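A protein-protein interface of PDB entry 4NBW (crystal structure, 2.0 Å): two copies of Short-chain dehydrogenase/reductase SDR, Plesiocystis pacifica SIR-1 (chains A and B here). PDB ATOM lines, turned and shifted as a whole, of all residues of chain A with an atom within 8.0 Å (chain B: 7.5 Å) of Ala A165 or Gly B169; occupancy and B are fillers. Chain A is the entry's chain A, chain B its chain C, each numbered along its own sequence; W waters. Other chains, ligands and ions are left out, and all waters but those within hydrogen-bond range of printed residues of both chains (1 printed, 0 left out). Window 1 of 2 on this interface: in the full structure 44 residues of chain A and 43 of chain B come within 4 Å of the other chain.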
ATOM      1  N   PHE A 115      32.392 -11.727   8.162  1.00  0.00           N
ATOM      2  CA  PHE A 115      31.544 -12.792   7.636  1.00  0.00           C
ATOM      3  C   PHE A 115      32.408 -13.955   7.167  1.00  0.00           C
ATOM      4  O   PHE A 115      32.156 -15.105   7.530  1.00  0.00           O
ATOM      5  CB  PHE A 115      30.684 -12.299   6.487  1.00  0.00           C
ATOM      6  CG  PHE A 115      29.771 -13.342   5.942  1.00  0.00           C
ATOM      7  CD1 PHE A 115      28.548 -13.590   6.552  1.00  0.00           C
ATOM      8  CD2 PHE A 115      30.139 -14.094   4.837  1.00  0.00           C
ATOM      9  CE1 PHE A 115      27.702 -14.544   6.062  1.00  0.00           C
ATOM     10  CE2 PHE A 115      29.295 -15.064   4.333  1.00  0.00           C
ATOM     11  CZ  PHE A 115      28.071 -15.299   4.943  1.00  0.00           C
ATOM     12  N   VAL A 118      34.398 -16.215   9.956  1.00  0.00           N
ATOM     13  CA  VAL A 118      33.606 -17.200  10.681  1.00  0.00           C
ATOM     14  C   VAL A 118      33.218 -18.385   9.751  1.00  0.00           C
ATOM     15  O   VAL A 118      33.287 -19.568  10.152  1.00  0.00           O
ATOM     16  CB  VAL A 118      32.384 -16.540  11.288  1.00  0.00           C
ATOM     17  CG1 VAL A 118      31.463 -17.571  11.865  1.00  0.00           C
ATOM     18  CG2 VAL A 118      32.839 -15.532  12.366  1.00  0.00           C
ATOM     19  N   ILE A 119      32.851 -18.069   8.511  1.00  0.00           N
ATOM     20  CA  ILE A 119      32.622 -19.105   7.506  1.00  0.00           C
ATOM     21  C   ILE A 119      33.849 -19.993   7.317  1.00  0.00           C
ATOM     22  O   ILE A 119      33.732 -21.209   7.262  1.00  0.00           O
ATOM     23  CB  ILE A 119      32.236 -18.512   6.122  1.00  0.00           C
ATOM     24  CG1 ILE A 119      30.909 -17.746   6.198  1.00  0.00           C
ATOM     25  CG2 ILE A 119      32.130 -19.620   5.039  1.00  0.00           C
ATOM     26  CD1 ILE A 119      29.731 -18.564   6.661  1.00  0.00           C
ATOM     27  N   ASN A 122      34.435 -22.107  10.772  1.00  0.00           N
ATOM     28  CA  ASN A 122      33.322 -22.859  11.334  1.00  0.00           C
ATOM     29  C   ASN A 122      32.599 -23.727  10.310  1.00  0.00           C
ATOM     30  O   ASN A 122      31.869 -24.670  10.670  1.00  0.00           O
ATOM     31  CB  ASN A 122      32.313 -21.907  11.986  1.00  0.00           C
ATOM     32  CG  ASN A 122      32.912 -21.111  13.105  1.00  0.00           C
ATOM     33  OD1 ASN A 122      34.108 -20.884  13.144  1.00  0.00           O
ATOM     34  ND2 ASN A 122      32.076 -20.674  14.019  1.00  0.00           N
ATOM     35  N   LEU A 123      32.762 -23.379   9.045  1.00  0.00           N
ATOM     36  CA  LEU A 123      32.122 -24.136   7.962  1.00  0.00           C
ATOM     37  C   LEU A 123      33.188 -24.810   7.110  1.00  0.00           C
ATOM     38  O   LEU A 123      33.225 -26.055   7.033  1.00  0.00           O
ATOM     39  CB  LEU A 123      31.221 -23.226   7.096  1.00  0.00           C
ATOM     40  CG  LEU A 123      30.358 -23.988   6.090  1.00  0.00           C
ATOM     41  CD1 LEU A 123      29.310 -24.835   6.835  1.00  0.00           C
ATOM     42  CD2 LEU A 123      29.682 -23.087   5.092  1.00  0.00           C
ATOM     43  N   VAL A 152      21.623 -22.430  18.134  1.00  0.00           N
ATOM     44  CA  VAL A 152      21.350 -21.221  17.374  1.00  0.00           C
ATOM     45  C   VAL A 152      21.325 -21.546  15.867  1.00  0.00           C
ATOM     46  O   VAL A 152      20.750 -20.802  15.037  1.00  0.00           O
ATOM     47  CB  VAL A 152      22.396 -20.170  17.807  1.00  0.00           C
ATOM     48  CG1 VAL A 152      23.077 -19.497  16.665  1.00  0.00           C
ATOM     49  CG2 VAL A 152      21.769 -19.205  18.813  1.00  0.00           C
ATOM     50  N   GLY A 153      21.869 -22.706  15.521  1.00  0.00           N
ATOM     51  CA  GLY A 153      21.753 -23.218  14.167  1.00  0.00           C
ATOM     52  C   GLY A 153      20.361 -23.727  13.834  1.00  0.00           C
ATOM     53  O   GLY A 153      19.998 -23.872  12.653  1.00  0.00           O
ATOM     54  N   GLY A 156      18.026 -19.721  14.694  1.00  0.00           N
ATOM     55  CA  GLY A 156      18.591 -18.436  14.371  1.00  0.00           C
ATOM     56  C   GLY A 156      18.739 -17.619  15.654  1.00  0.00           C
ATOM     57  O   GLY A 156      18.280 -18.031  16.719  1.00  0.00           O
ATOM     58  N   GLN A 160      23.860 -12.680  14.663  1.00  0.00           N
ATOM     59  CA  GLN A 160      24.746 -13.794  14.321  1.00  0.00           C
ATOM     60  C   GLN A 160      24.567 -14.316  12.877  1.00  0.00           C
ATOM     61  O   GLN A 160      24.635 -15.526  12.650  1.00  0.00           O
ATOM     62  CB  GLN A 160      24.524 -14.951  15.298  1.00  0.00           C
ATOM     63  CG  GLN A 160      24.701 -14.552  16.780  1.00  0.00           C
ATOM     64  CD  GLN A 160      25.056 -15.725  17.655  1.00  0.00           C
ATOM     65  OE1 GLN A 160      24.186 -16.403  18.181  1.00  0.00           O
ATOM     66  NE2 GLN A 160      26.352 -15.960  17.827  1.00  0.00           N
ATOM     67  N   THR A 161      24.346 -13.409  11.918  1.00  0.00           N
ATOM     68  CA  THR A 161      24.295 -13.790  10.493  1.00  0.00           C
ATOM     69  C   THR A 161      25.344 -14.872  10.148  1.00  0.00           C
ATOM     70  O   THR A 161      24.996 -15.930   9.614  1.00  0.00           O
ATOM     71  CB  THR A 161      24.535 -12.577   9.582  1.00  0.00           C
ATOM     72  OG1 THR A 161      23.460 -11.629   9.716  1.00  0.00           O
ATOM     73  CG2 THR A 161      24.661 -13.003   8.114  1.00  0.00           C
ATOM     74  N   ASN A 162      26.614 -14.598  10.475  1.00  0.00           N
ATOM     75  CA  ASN A 162      27.734 -15.470  10.082  1.00  0.00           C
ATOM     76  C   ASN A 162      27.781 -16.791  10.850  1.00  0.00           C
ATOM     77  O   ASN A 162      27.923 -17.876  10.271  1.00  0.00           O
ATOM     78  CB  ASN A 162      29.092 -14.736  10.227  1.00  0.00           C
ATOM     79  CG  ASN A 162      29.258 -13.982  11.555  1.00  0.00           C
ATOM     80  OD1 ASN A 162      28.437 -14.055  12.451  1.00  0.00           O
ATOM     81  ND2 ASN A 162      30.346 -13.251  11.664  1.00  0.00           N
ATOM     82  N   TYR A 163      27.664 -16.700  12.159  1.00  0.00           N
ATOM     83  CA  TYR A 163      27.780 -17.883  13.004  1.00  0.00           C
ATOM     84  C   TYR A 163      26.618 -18.837  12.699  1.00  0.00           C
ATOM     85  O   TYR A 163      26.816 -20.036  12.560  1.00  0.00           O
ATOM     86  CB  TYR A 163      27.795 -17.462  14.471  1.00  0.00           C
ATOM     87  CG  TYR A 163      28.145 -18.530  15.476  1.00  0.00           C
ATOM     88  CD1 TYR A 163      29.452 -18.896  15.701  1.00  0.00           C
ATOM     89  CD2 TYR A 163      27.155 -19.144  16.226  1.00  0.00           C
ATOM     90  CE1 TYR A 163      29.761 -19.829  16.646  1.00  0.00           C
ATOM     91  CE2 TYR A 163      27.444 -20.091  17.141  1.00  0.00           C
ATOM     92  CZ  TYR A 163      28.748 -20.427  17.359  1.00  0.00           C
ATOM     93  OH  TYR A 163      29.044 -21.372  18.318  1.00  0.00           O
ATOM     94  N   VAL A 164      25.410 -18.297  12.557  1.00  0.00           N
ATOM     95  CA  VAL A 164      24.239 -19.131  12.259  1.00  0.00           C
ATOM     96  C   VAL A 164      24.324 -19.780  10.864  1.00  0.00           C
ATOM     97  O   VAL A 164      23.865 -20.881  10.666  1.00  0.00           O
ATOM     98  CB  VAL A 164      22.944 -18.315  12.350  1.00  0.00           C
ATOM     99  CG1 VAL A 164      21.737 -19.080  11.748  1.00  0.00           C
ATOM    100  CG2 VAL A 164      22.675 -17.958  13.777  1.00  0.00           C
ATOM    101  N   ALA A 165      24.875 -19.073   9.887  1.00  0.00           N
ATOM    102  CA  ALA A 165      25.023 -19.638   8.538  1.00  0.00           C
ATOM    103  C   ALA A 165      25.909 -20.877   8.591  1.00  0.00           C
ATOM    104  O   ALA A 165      25.607 -21.896   7.983  1.00  0.00           O
ATOM    105  CB  ALA A 165      25.627 -18.621   7.607  1.00  0.00           C
ATOM    106  N   ALA A 166      27.021 -20.737   9.319  1.00  0.00           N
ATOM    107  CA  ALA A 166      28.010 -21.800   9.522  1.00  0.00           C
ATOM    108  C   ALA A 166      27.397 -22.972  10.247  1.00  0.00           C
ATOM    109  O   ALA A 166      27.573 -24.129   9.836  1.00  0.00           O
ATOM    110  CB  ALA A 166      29.184 -21.290  10.313  1.00  0.00           C
ATOM    111  N   LYS A 167      26.699 -22.676  11.340  1.00  0.00           N
ATOM    112  CA  LYS A 167      26.230 -23.742  12.211  1.00  0.00           C
ATOM    113  C   LYS A 167      25.043 -24.480  11.601  1.00  0.00           C
ATOM    114  O   LYS A 167      24.934 -25.704  11.790  1.00  0.00           O
ATOM    115  CB  LYS A 167      25.875 -23.216  13.607  1.00  0.00           C
ATOM    116  CG  LYS A 167      27.050 -22.640  14.350  1.00  0.00           C
ATOM    117  CD  LYS A 167      28.189 -23.659  14.470  1.00  0.00           C
ATOM    118  CE  LYS A 167      29.436 -23.015  15.015  1.00  0.00           C
ATOM    119  NZ  LYS A 167      30.567 -23.997  15.114  1.00  0.00           N
ATOM    120  N   SER A 168      24.192 -23.772  10.855  1.00  0.00           N
ATOM    121  CA  SER A 168      23.119 -24.430  10.100  1.00  0.00           C
ATOM    122  C   SER A 168      23.683 -25.243   8.938  1.00  0.00           C
ATOM    123  O   SER A 168      23.212 -26.347   8.635  1.00  0.00           O
ATOM    124  CB  SER A 168      22.086 -23.411   9.586  1.00  0.00           C
ATOM    125  OG  SER A 168      22.688 -22.285   8.970  1.00  0.00           O
ATOM    126  N   GLY A 169      24.720 -24.736   8.293  1.00  0.00           N
ATOM    127  CA  GLY A 169      25.294 -25.452   7.174  1.00  0.00           C
ATOM    128  C   GLY A 169      26.046 -26.689   7.610  1.00  0.00           C
ATOM    129  O   GLY A 169      26.096 -27.673   6.875  1.00  0.00           O
ATOM    130  N   VAL A 170      26.616 -26.650   8.822  1.00  0.00           N
ATOM    131  CA  VAL A 170      27.343 -27.790   9.372  1.00  0.00           C
ATOM    132  C   VAL A 170      26.374 -28.970   9.523  1.00  0.00           C
ATOM    133  O   VAL A 170      26.700 -30.104   9.222  1.00  0.00           O
ATOM    134  CB  VAL A 170      28.013 -27.423  10.734  1.00  0.00           C
ATOM    135  CG1 VAL A 170      28.212 -28.664  11.589  1.00  0.00           C
ATOM    136  CG2 VAL A 170      29.336 -26.727  10.497  1.00  0.00           C
ATOM    137  N   ILE A 171      25.150 -28.682   9.936  1.00  0.00           N
ATOM    138  CA  ILE A 171      24.114 -29.712   9.996  1.00  0.00           C
ATOM    139  C   ILE A 171      23.827 -30.256   8.582  1.00  0.00           C
ATOM    140  O   ILE A 171      23.628 -31.450   8.397  1.00  0.00           O
ATOM    141  CB  ILE A 171      22.859 -29.147  10.665  1.00  0.00           C
ATOM    142  CG1 ILE A 171      23.166 -28.916  12.151  1.00  0.00           C
ATOM    143  CG2 ILE A 171      21.663 -30.085  10.518  1.00  0.00           C
ATOM    144  CD1 ILE A 171      22.166 -28.051  12.856  1.00  0.00           C
ATOM    145  N   GLY A 172      23.878 -29.395   7.576  1.00  0.00           N
ATOM    146  CA  GLY A 172      23.585 -29.833   6.220  1.00  0.00           C
ATOM    147  C   GLY A 172      24.633 -30.819   5.751  1.00  0.00           C
ATOM    148  O   GLY A 172      24.303 -31.904   5.200  1.00  0.00           O
ATOM    149  N   ASN B 122      26.118 -18.892  -3.654  1.00  0.00           N
ATOM    150  CA  ASN B 122      24.908 -19.348  -3.034  1.00  0.00           C
ATOM    151  C   ASN B 122      24.719 -18.946  -1.572  1.00  0.00           C
ATOM    152  O   ASN B 122      23.612 -19.046  -1.050  1.00  0.00           O
ATOM    153  CB  ASN B 122      24.837 -20.866  -3.127  1.00  0.00           C
ATOM    154  CG  ASN B 122      24.867 -21.377  -4.551  1.00  0.00           C
ATOM    155  OD1 ASN B 122      25.401 -20.738  -5.460  1.00  0.00           O
ATOM    156  ND2 ASN B 122      24.283 -22.548  -4.754  1.00  0.00           N
ATOM    157  N   LEU B 123      25.774 -18.532  -0.886  1.00  0.00           N
ATOM    158  CA  LEU B 123      25.630 -18.150   0.531  1.00  0.00           C
ATOM    159  C   LEU B 123      26.102 -16.708   0.711  1.00  0.00           C
ATOM    160  O   LEU B 123      25.327 -15.878   1.151  1.00  0.00           O
ATOM    161  CB  LEU B 123      26.404 -19.113   1.467  1.00  0.00           C
ATOM    162  CG  LEU B 123      26.200 -18.837   2.964  1.00  0.00           C
ATOM    163  CD1 LEU B 123      24.868 -19.430   3.443  1.00  0.00           C
ATOM    164  CD2 LEU B 123      27.360 -19.370   3.805  1.00  0.00           C
ATOM    165  N   VAL B 126      24.004 -14.093  -1.109  1.00  0.00           N
ATOM    166  CA  VAL B 126      22.732 -13.800  -0.470  1.00  0.00           C
ATOM    167  C   VAL B 126      22.972 -12.771   0.651  1.00  0.00           C
ATOM    168  O   VAL B 126      22.205 -11.819   0.819  1.00  0.00           O
ATOM    169  CB  VAL B 126      22.055 -15.091   0.070  1.00  0.00           C
ATOM    170  CG1 VAL B 126      20.763 -14.778   0.743  1.00  0.00           C
ATOM    171  CG2 VAL B 126      21.795 -16.077  -1.056  1.00  0.00           C
ATOM    172  N   SER B 149      16.343 -21.233  -1.208  1.00  0.00           N
ATOM    173  CA  SER B 149      16.908 -22.406  -0.568  1.00  0.00           C
ATOM    174  C   SER B 149      16.614 -23.600  -1.479  1.00  0.00           C
ATOM    175  O   SER B 149      16.466 -23.432  -2.699  1.00  0.00           O
ATOM    176  CB  SER B 149      16.350 -22.619   0.831  1.00  0.00           C
ATOM    177  OG  SER B 149      17.018 -23.701   1.418  1.00  0.00           O
ATOM    178  N   GLY B 153      18.266 -28.602   1.231  1.00  0.00           N
ATOM    179  CA  GLY B 153      18.675 -27.932   2.461  1.00  0.00           C
ATOM    180  C   GLY B 153      18.013 -28.544   3.686  1.00  0.00           C
ATOM    181  O   GLY B 153      18.502 -28.404   4.811  1.00  0.00           O
ATOM    182  N   TYR B 163      26.563 -27.570  -1.977  1.00  0.00           N
ATOM    183  CA  TYR B 163      25.273 -26.988  -2.309  1.00  0.00           C
ATOM    184  C   TYR B 163      24.358 -27.039  -1.105  1.00  0.00           C
ATOM    185  O   TYR B 163      23.657 -26.082  -0.837  1.00  0.00           O
ATOM    186  CB  TYR B 163      24.614 -27.725  -3.482  1.00  0.00           C
ATOM    187  CG  TYR B 163      23.405 -27.026  -4.088  1.00  0.00           C
ATOM    188  CD1 TYR B 163      23.558 -25.975  -4.950  1.00  0.00           C
ATOM    189  CD2 TYR B 163      22.117 -27.452  -3.806  1.00  0.00           C
ATOM    190  CE1 TYR B 163      22.455 -25.375  -5.533  1.00  0.00           C
ATOM    191  CE2 TYR B 163      21.018 -26.859  -4.371  1.00  0.00           C
ATOM    192  CZ  TYR B 163      21.194 -25.825  -5.233  1.00  0.00           C
ATOM    193  OH  TYR B 163      20.097 -25.223  -5.813  1.00  0.00           O
ATOM    194  N   VAL B 164      24.388 -28.153  -0.381  1.00  0.00           N
ATOM    195  CA  VAL B 164      23.584 -28.313   0.849  1.00  0.00           C
ATOM    196  C   VAL B 164      23.994 -27.404   2.008  1.00  0.00           C
ATOM    197  O   VAL B 164      23.151 -26.927   2.759  1.00  0.00           O
ATOM    198  CB  VAL B 164      23.662 -29.745   1.335  1.00  0.00           C
ATOM    199  CG1 VAL B 164      23.101 -29.902   2.792  1.00  0.00           C
ATOM    200  CG2 VAL B 164      22.919 -30.614   0.376  1.00  0.00           C
ATOM    201  N   ALA B 165      25.303 -27.214   2.166  1.00  0.00           N
ATOM    202  CA  ALA B 165      25.847 -26.301   3.152  1.00  0.00           C
ATOM    203  C   ALA B 165      25.278 -24.916   2.930  1.00  0.00           C
ATOM    204  O   ALA B 165      24.831 -24.256   3.866  1.00  0.00           O
ATOM    205  CB  ALA B 165      27.389 -26.272   3.064  1.00  0.00           C
ATOM    206  N   ALA B 166      25.301 -24.472   1.677  1.00  0.00           N
ATOM    207  CA  ALA B 166      24.868 -23.118   1.341  1.00  0.00           C
ATOM    208  C   ALA B 166      23.368 -22.947   1.488  1.00  0.00           C
ATOM    209  O   ALA B 166      22.907 -21.895   1.936  1.00  0.00           O
ATOM    210  CB  ALA B 166      25.289 -22.764  -0.063  1.00  0.00           C
ATOM    211  N   LYS B 167      22.594 -23.947   1.140  1.00  0.00           N
ATOM    212  CA  LYS B 167      21.151 -23.842   1.117  1.00  0.00           C
ATOM    213  C   LYS B 167      20.570 -24.025   2.546  1.00  0.00           C
ATOM    214  O   LYS B 167      19.680 -23.335   2.930  1.00  0.00           O
ATOM    215  CB  LYS B 167      20.541 -24.850   0.126  1.00  0.00           C
ATOM    216  CG  LYS B 167      20.933 -24.599  -1.333  1.00  0.00           C
ATOM    217  CD  LYS B 167      20.474 -23.257  -1.877  1.00  0.00           C
ATOM    218  CE  LYS B 167      20.937 -22.844  -3.237  1.00  0.00           C
ATOM    219  NZ  LYS B 167      20.276 -21.658  -3.785  1.00  0.00           N
ATOM    220  N   SER B 168      21.164 -24.915   3.322  1.00  0.00           N
ATOM    221  CA  SER B 168      20.772 -24.989   4.732  1.00  0.00           C
ATOM    222  C   SER B 168      21.221 -23.710   5.442  1.00  0.00           C
ATOM    223  O   SER B 168      20.530 -23.178   6.324  1.00  0.00           O
ATOM    224  CB  SER B 168      21.362 -26.222   5.418  1.00  0.00           C
ATOM    225  OG  SER B 168      22.753 -26.211   5.301  1.00  0.00           O
ATOM    226  N   GLY B 169      22.371 -23.192   5.045  1.00  0.00           N
ATOM    227  CA  GLY B 169      22.896 -21.984   5.653  1.00  0.00           C
ATOM    228  C   GLY B 169      22.100 -20.727   5.289  1.00  0.00           C
ATOM    229  O   GLY B 169      22.017 -19.785   6.089  1.00  0.00           O
ATOM    230  N   VAL B 170      21.550 -20.706   4.069  1.00  0.00           N
ATOM    231  CA  VAL B 170      20.627 -19.639   3.649  1.00  0.00           C
ATOM    232  C   VAL B 170      19.386 -19.611   4.563  1.00  0.00           C
ATOM    233  O   VAL B 170      18.927 -18.536   4.950  1.00  0.00           O
ATOM    234  CB  VAL B 170      20.224 -19.788   2.144  1.00  0.00           C
ATOM    235  CG1 VAL B 170      18.985 -18.997   1.801  1.00  0.00           C
ATOM    236  CG2 VAL B 170      21.365 -19.275   1.294  1.00  0.00           C
ATOM    237  N   ILE B 171      18.852 -20.776   4.923  1.00  0.00           N
ATOM    238  CA  ILE B 171      17.717 -20.826   5.837  1.00  0.00           C
ATOM    239  C   ILE B 171      18.102 -20.218   7.190  1.00  0.00           C
ATOM    240  O   ILE B 171      17.312 -19.477   7.813  1.00  0.00           O
ATOM    241  CB  ILE B 171      17.228 -22.251   6.035  1.00  0.00           C
ATOM    242  CG1 ILE B 171      16.623 -22.782   4.727  1.00  0.00           C
ATOM    243  CG2 ILE B 171      16.176 -22.317   7.194  1.00  0.00           C
ATOM    244  CD1 ILE B 171      16.308 -24.214   4.792  1.00  0.00           C
ATOM    245  N   GLY B 172      19.336 -20.472   7.618  1.00  0.00           N
ATOM    246  CA  GLY B 172      19.817 -19.930   8.888  1.00  0.00           C
ATOM    247  C   GLY B 172      19.852 -18.416   8.895  1.00  0.00           C
ATOM    248  O   GLY B 172      19.422 -17.759   9.871  1.00  0.00           O
ATOM    249  N   MET B 173      20.398 -17.847   7.823  1.00  0.00           N
ATOM    250  CA  MET B 173      20.458 -16.403   7.697  1.00  0.00           C
ATOM    251  C   MET B 173      19.051 -15.804   7.609  1.00  0.00           C
ATOM    252  O   MET B 173      18.814 -14.709   8.106  1.00  0.00           O
ATOM    253  CB  MET B 173      21.281 -15.994   6.472  1.00  0.00           C
ATOM    254  CG  MET B 173      22.676 -16.452   6.517  1.00  0.00           C
ATOM    255  SD  MET B 173      23.826 -15.604   5.399  1.00  0.00           S
ATOM    256  CE  MET B 173      23.084 -16.133   3.856  1.00  0.00           C
ATOM    257  N   THR B 174      18.134 -16.526   6.957  1.00  0.00           N
ATOM    258  CA  THR B 174      16.753 -16.092   6.825  1.00  0.00           C
ATOM    259  C   THR B 174      16.169 -15.901   8.226  1.00  0.00           C
ATOM    260  O   THR B 174      15.497 -14.891   8.508  1.00  0.00           O
ATOM    261  CB  THR B 174      15.897 -17.097   6.010  1.00  0.00           C
ATOM    262  OG1 THR B 174      16.469 -17.299   4.708  1.00  0.00           O
ATOM    263  CG2 THR B 174      14.487 -16.578   5.822  1.00  0.00           C
ATOM    264  N   LYS B 175      16.481 -16.821   9.130  1.00  0.00           N
ATOM    265  CA  LYS B 175      15.981 -16.712  10.505  1.00  0.00           C
ATOM    266  C   LYS B 175      16.619 -15.539  11.267  1.00  0.00           C
ATOM    267  O   LYS B 175      15.917 -14.820  11.966  1.00  0.00           O
ATOM    268  CB  LYS B 175      16.197 -18.021  11.250  1.00  0.00           C
ATOM    269  CG  LYS B 175      15.375 -19.170  10.696  1.00  0.00           C
ATOM    270  CD  LYS B 175      15.831 -20.501  11.304  1.00  0.00           C
ATOM    271  CE  LYS B 175      15.016 -21.684  10.778  1.00  0.00           C
ATOM    272  NZ  LYS B 175      15.652 -22.993  11.174  1.00  0.00           N
ATOM    273  N   VAL B 176      17.920 -15.316  11.103  1.00  0.00           N
ATOM    274  CA  VAL B 176      18.567 -14.162  11.731  1.00  0.00           C
ATOM    275  C   VAL B 176      17.854 -12.882  11.285  1.00  0.00           C
ATOM    276  O   VAL B 176      17.326 -12.129  12.097  1.00  0.00           O
ATOM    277  CB  VAL B 176      20.080 -14.053  11.372  1.00  0.00           C
ATOM    278  CG1 VAL B 176      20.691 -12.839  12.033  1.00  0.00           C
ATOM    279  CG2 VAL B 176      20.863 -15.327  11.808  1.00  0.00           C
ATOM    280  N   TRP B 177      17.803 -12.686   9.978  1.00  0.00           N
ATOM    281  CA  TRP B 177      17.379 -11.426   9.413  1.00  0.00           C
ATOM    282  C   TRP B 177      15.932 -11.109   9.736  1.00  0.00           C
ATOM    283  O   TRP B 177      15.589  -9.945  10.019  1.00  0.00           O
ATOM    284  CB  TRP B 177      17.615 -11.444   7.922  1.00  0.00           C
ATOM    285  CG  TRP B 177      19.045 -11.556   7.582  1.00  0.00           C
ATOM    286  CD1 TRP B 177      20.117 -11.275   8.398  1.00  0.00           C
ATOM    287  CD2 TRP B 177      19.591 -11.999   6.338  1.00  0.00           C
ATOM    288  NE1 TRP B 177      21.298 -11.513   7.722  1.00  0.00           N
ATOM    289  CE2 TRP B 177      20.998 -11.941   6.453  1.00  0.00           C
ATOM    290  CE3 TRP B 177      19.033 -12.428   5.133  1.00  0.00           C
ATOM    291  CZ2 TRP B 177      21.844 -12.306   5.407  1.00  0.00           C
ATOM    292  CZ3 TRP B 177      19.874 -12.787   4.094  1.00  0.00           C
ATOM    293  CH2 TRP B 177      21.265 -12.728   4.239  1.00  0.00           C
HETATM  294  O   HOH W   1      18.013 -23.105  10.349  1.00  0.00           O
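Ile A119 touches Leu B123 (CD1 to CD2, 3.8 Å).
Gly A156 touches Lys B175.
Gln A160 touches Val B176.
Val B176 touches Thr A161 (CG1 to N, 3.7 Å).
CB of Val A164 touches CG2 of Val B176, at 3.7 Å.
Ala A165 touches Met B173.
CA of Gly B169 touches OG of Ser A168, at 3.3 Å.
Ser A168 touches Gly B172 (OG to CA, 3.7 Å).
OG of Ser B168 touches CA of Gly A169, 3.2 Å away.
Gly A172 touches Val B164 (O to CG1, 3.4 Å).
Water W1 lies within hydrogen-bond range of the side-chain amino group (NZ) of Lys B175 (2.5 Å) and the backbone carbonyl oxygen (O) of Gly A153 (3.1 Å).
Val A164 touches Gly B172, and with the chains exchanged Gly A172 touches Val B164.
Ala A165 touches Gly B169, and with the chains exchanged Gly A169 touches Ala B165.
Ser B168 touches its own counterpart, Ser A168.
Ser A168 touches Gly B172, and with the chains exchanged Gly A172 touches Ser B168.
13 positions are printed for both chains.
Of chain B, only Gly B169 and Met B173 come within 4 Å of Ala A165.
Of the printed residues of chain A, Gly B169 touches Ala A165 (3.6 Å) and Ser A168 (3.3 Å).
Of the printed residues of chain B, Gly A169 touches Ala B165 (3.5 Å) and Ser B168 (3.2 Å).
Of the printed residues of chain A, Met B173 touches Thr A161 and Ala A165.
Gly A153 touches none of the printed residues of chain B.
Val A152 touches none of the printed residues of chain B.
The nearest residue of chain B that does not touch Ala A165 is Leu B123 (4.2 Å).
The nearest residue of chain A that does not touch Gly B169 is Gly A169 (4.2 Å).
The nearest printed residue of chain B that does not touch Val A164 is Met B173 (4.3 Å).
Of the 21 printed residues of chain A, 9 touch a printed residue of chain B.
Printed residues of chain A that touch a printed residue of chain B: Ile A119, Gly A156, Gln A160, Thr A161, Val A164, Ala A165, Ser A168, Gly A169 and Gly A172.
Of the 20 printed residues of chain B, 10 touch a printed residue of chain A.
Printed residues of chain B that touch a printed residue of chain A: Leu B123, Val B164, Ala B165, Ser B168, Gly B169, Gly B172, Met B173, Lys B175, Val B176 and Trp B177.
Hydrophobic or aromatic side chains of chain B that line the printed part of chain A: Leu B123, Val B164, Met B173, Val B176 and Trp B177.
Along chain B the printed residues that touch a printed residue of chain A span positions 123 to 177.
Among the printed residues, no Asp or Glu carboxylate lies within 4 Å of a Lys or Arg side-chain nitrogen of the other chain.
The backbone carbonyl oxygen (O) of Ser A168 lies within hydrogen-bond range of the side-chain hydroxyl (OG) of Ser B168 (3.4 Å).
The side-chain hydroxyl (OG1) of Thr A161 lies within hydrogen-bond range of the indole nitrogen (NE1) of Trp B177, at 2.9 Å.
O of Ala A165 is in hydrogen-bond range of OG of Ser A168 (3.1 Å).
OG of Ser A168 is in hydrogen-bond range of O of Val A164 (2.5 Å).
OG of Ser B168 lies within hydrogen-bond range of O of Val B164, at 2.7 Å.
The backbone carbonyl oxygen (O) of Ala B165 lies within hydrogen-bond range of the side-chain hydroxyl (OG) of Ser B168 (3.2 Å).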
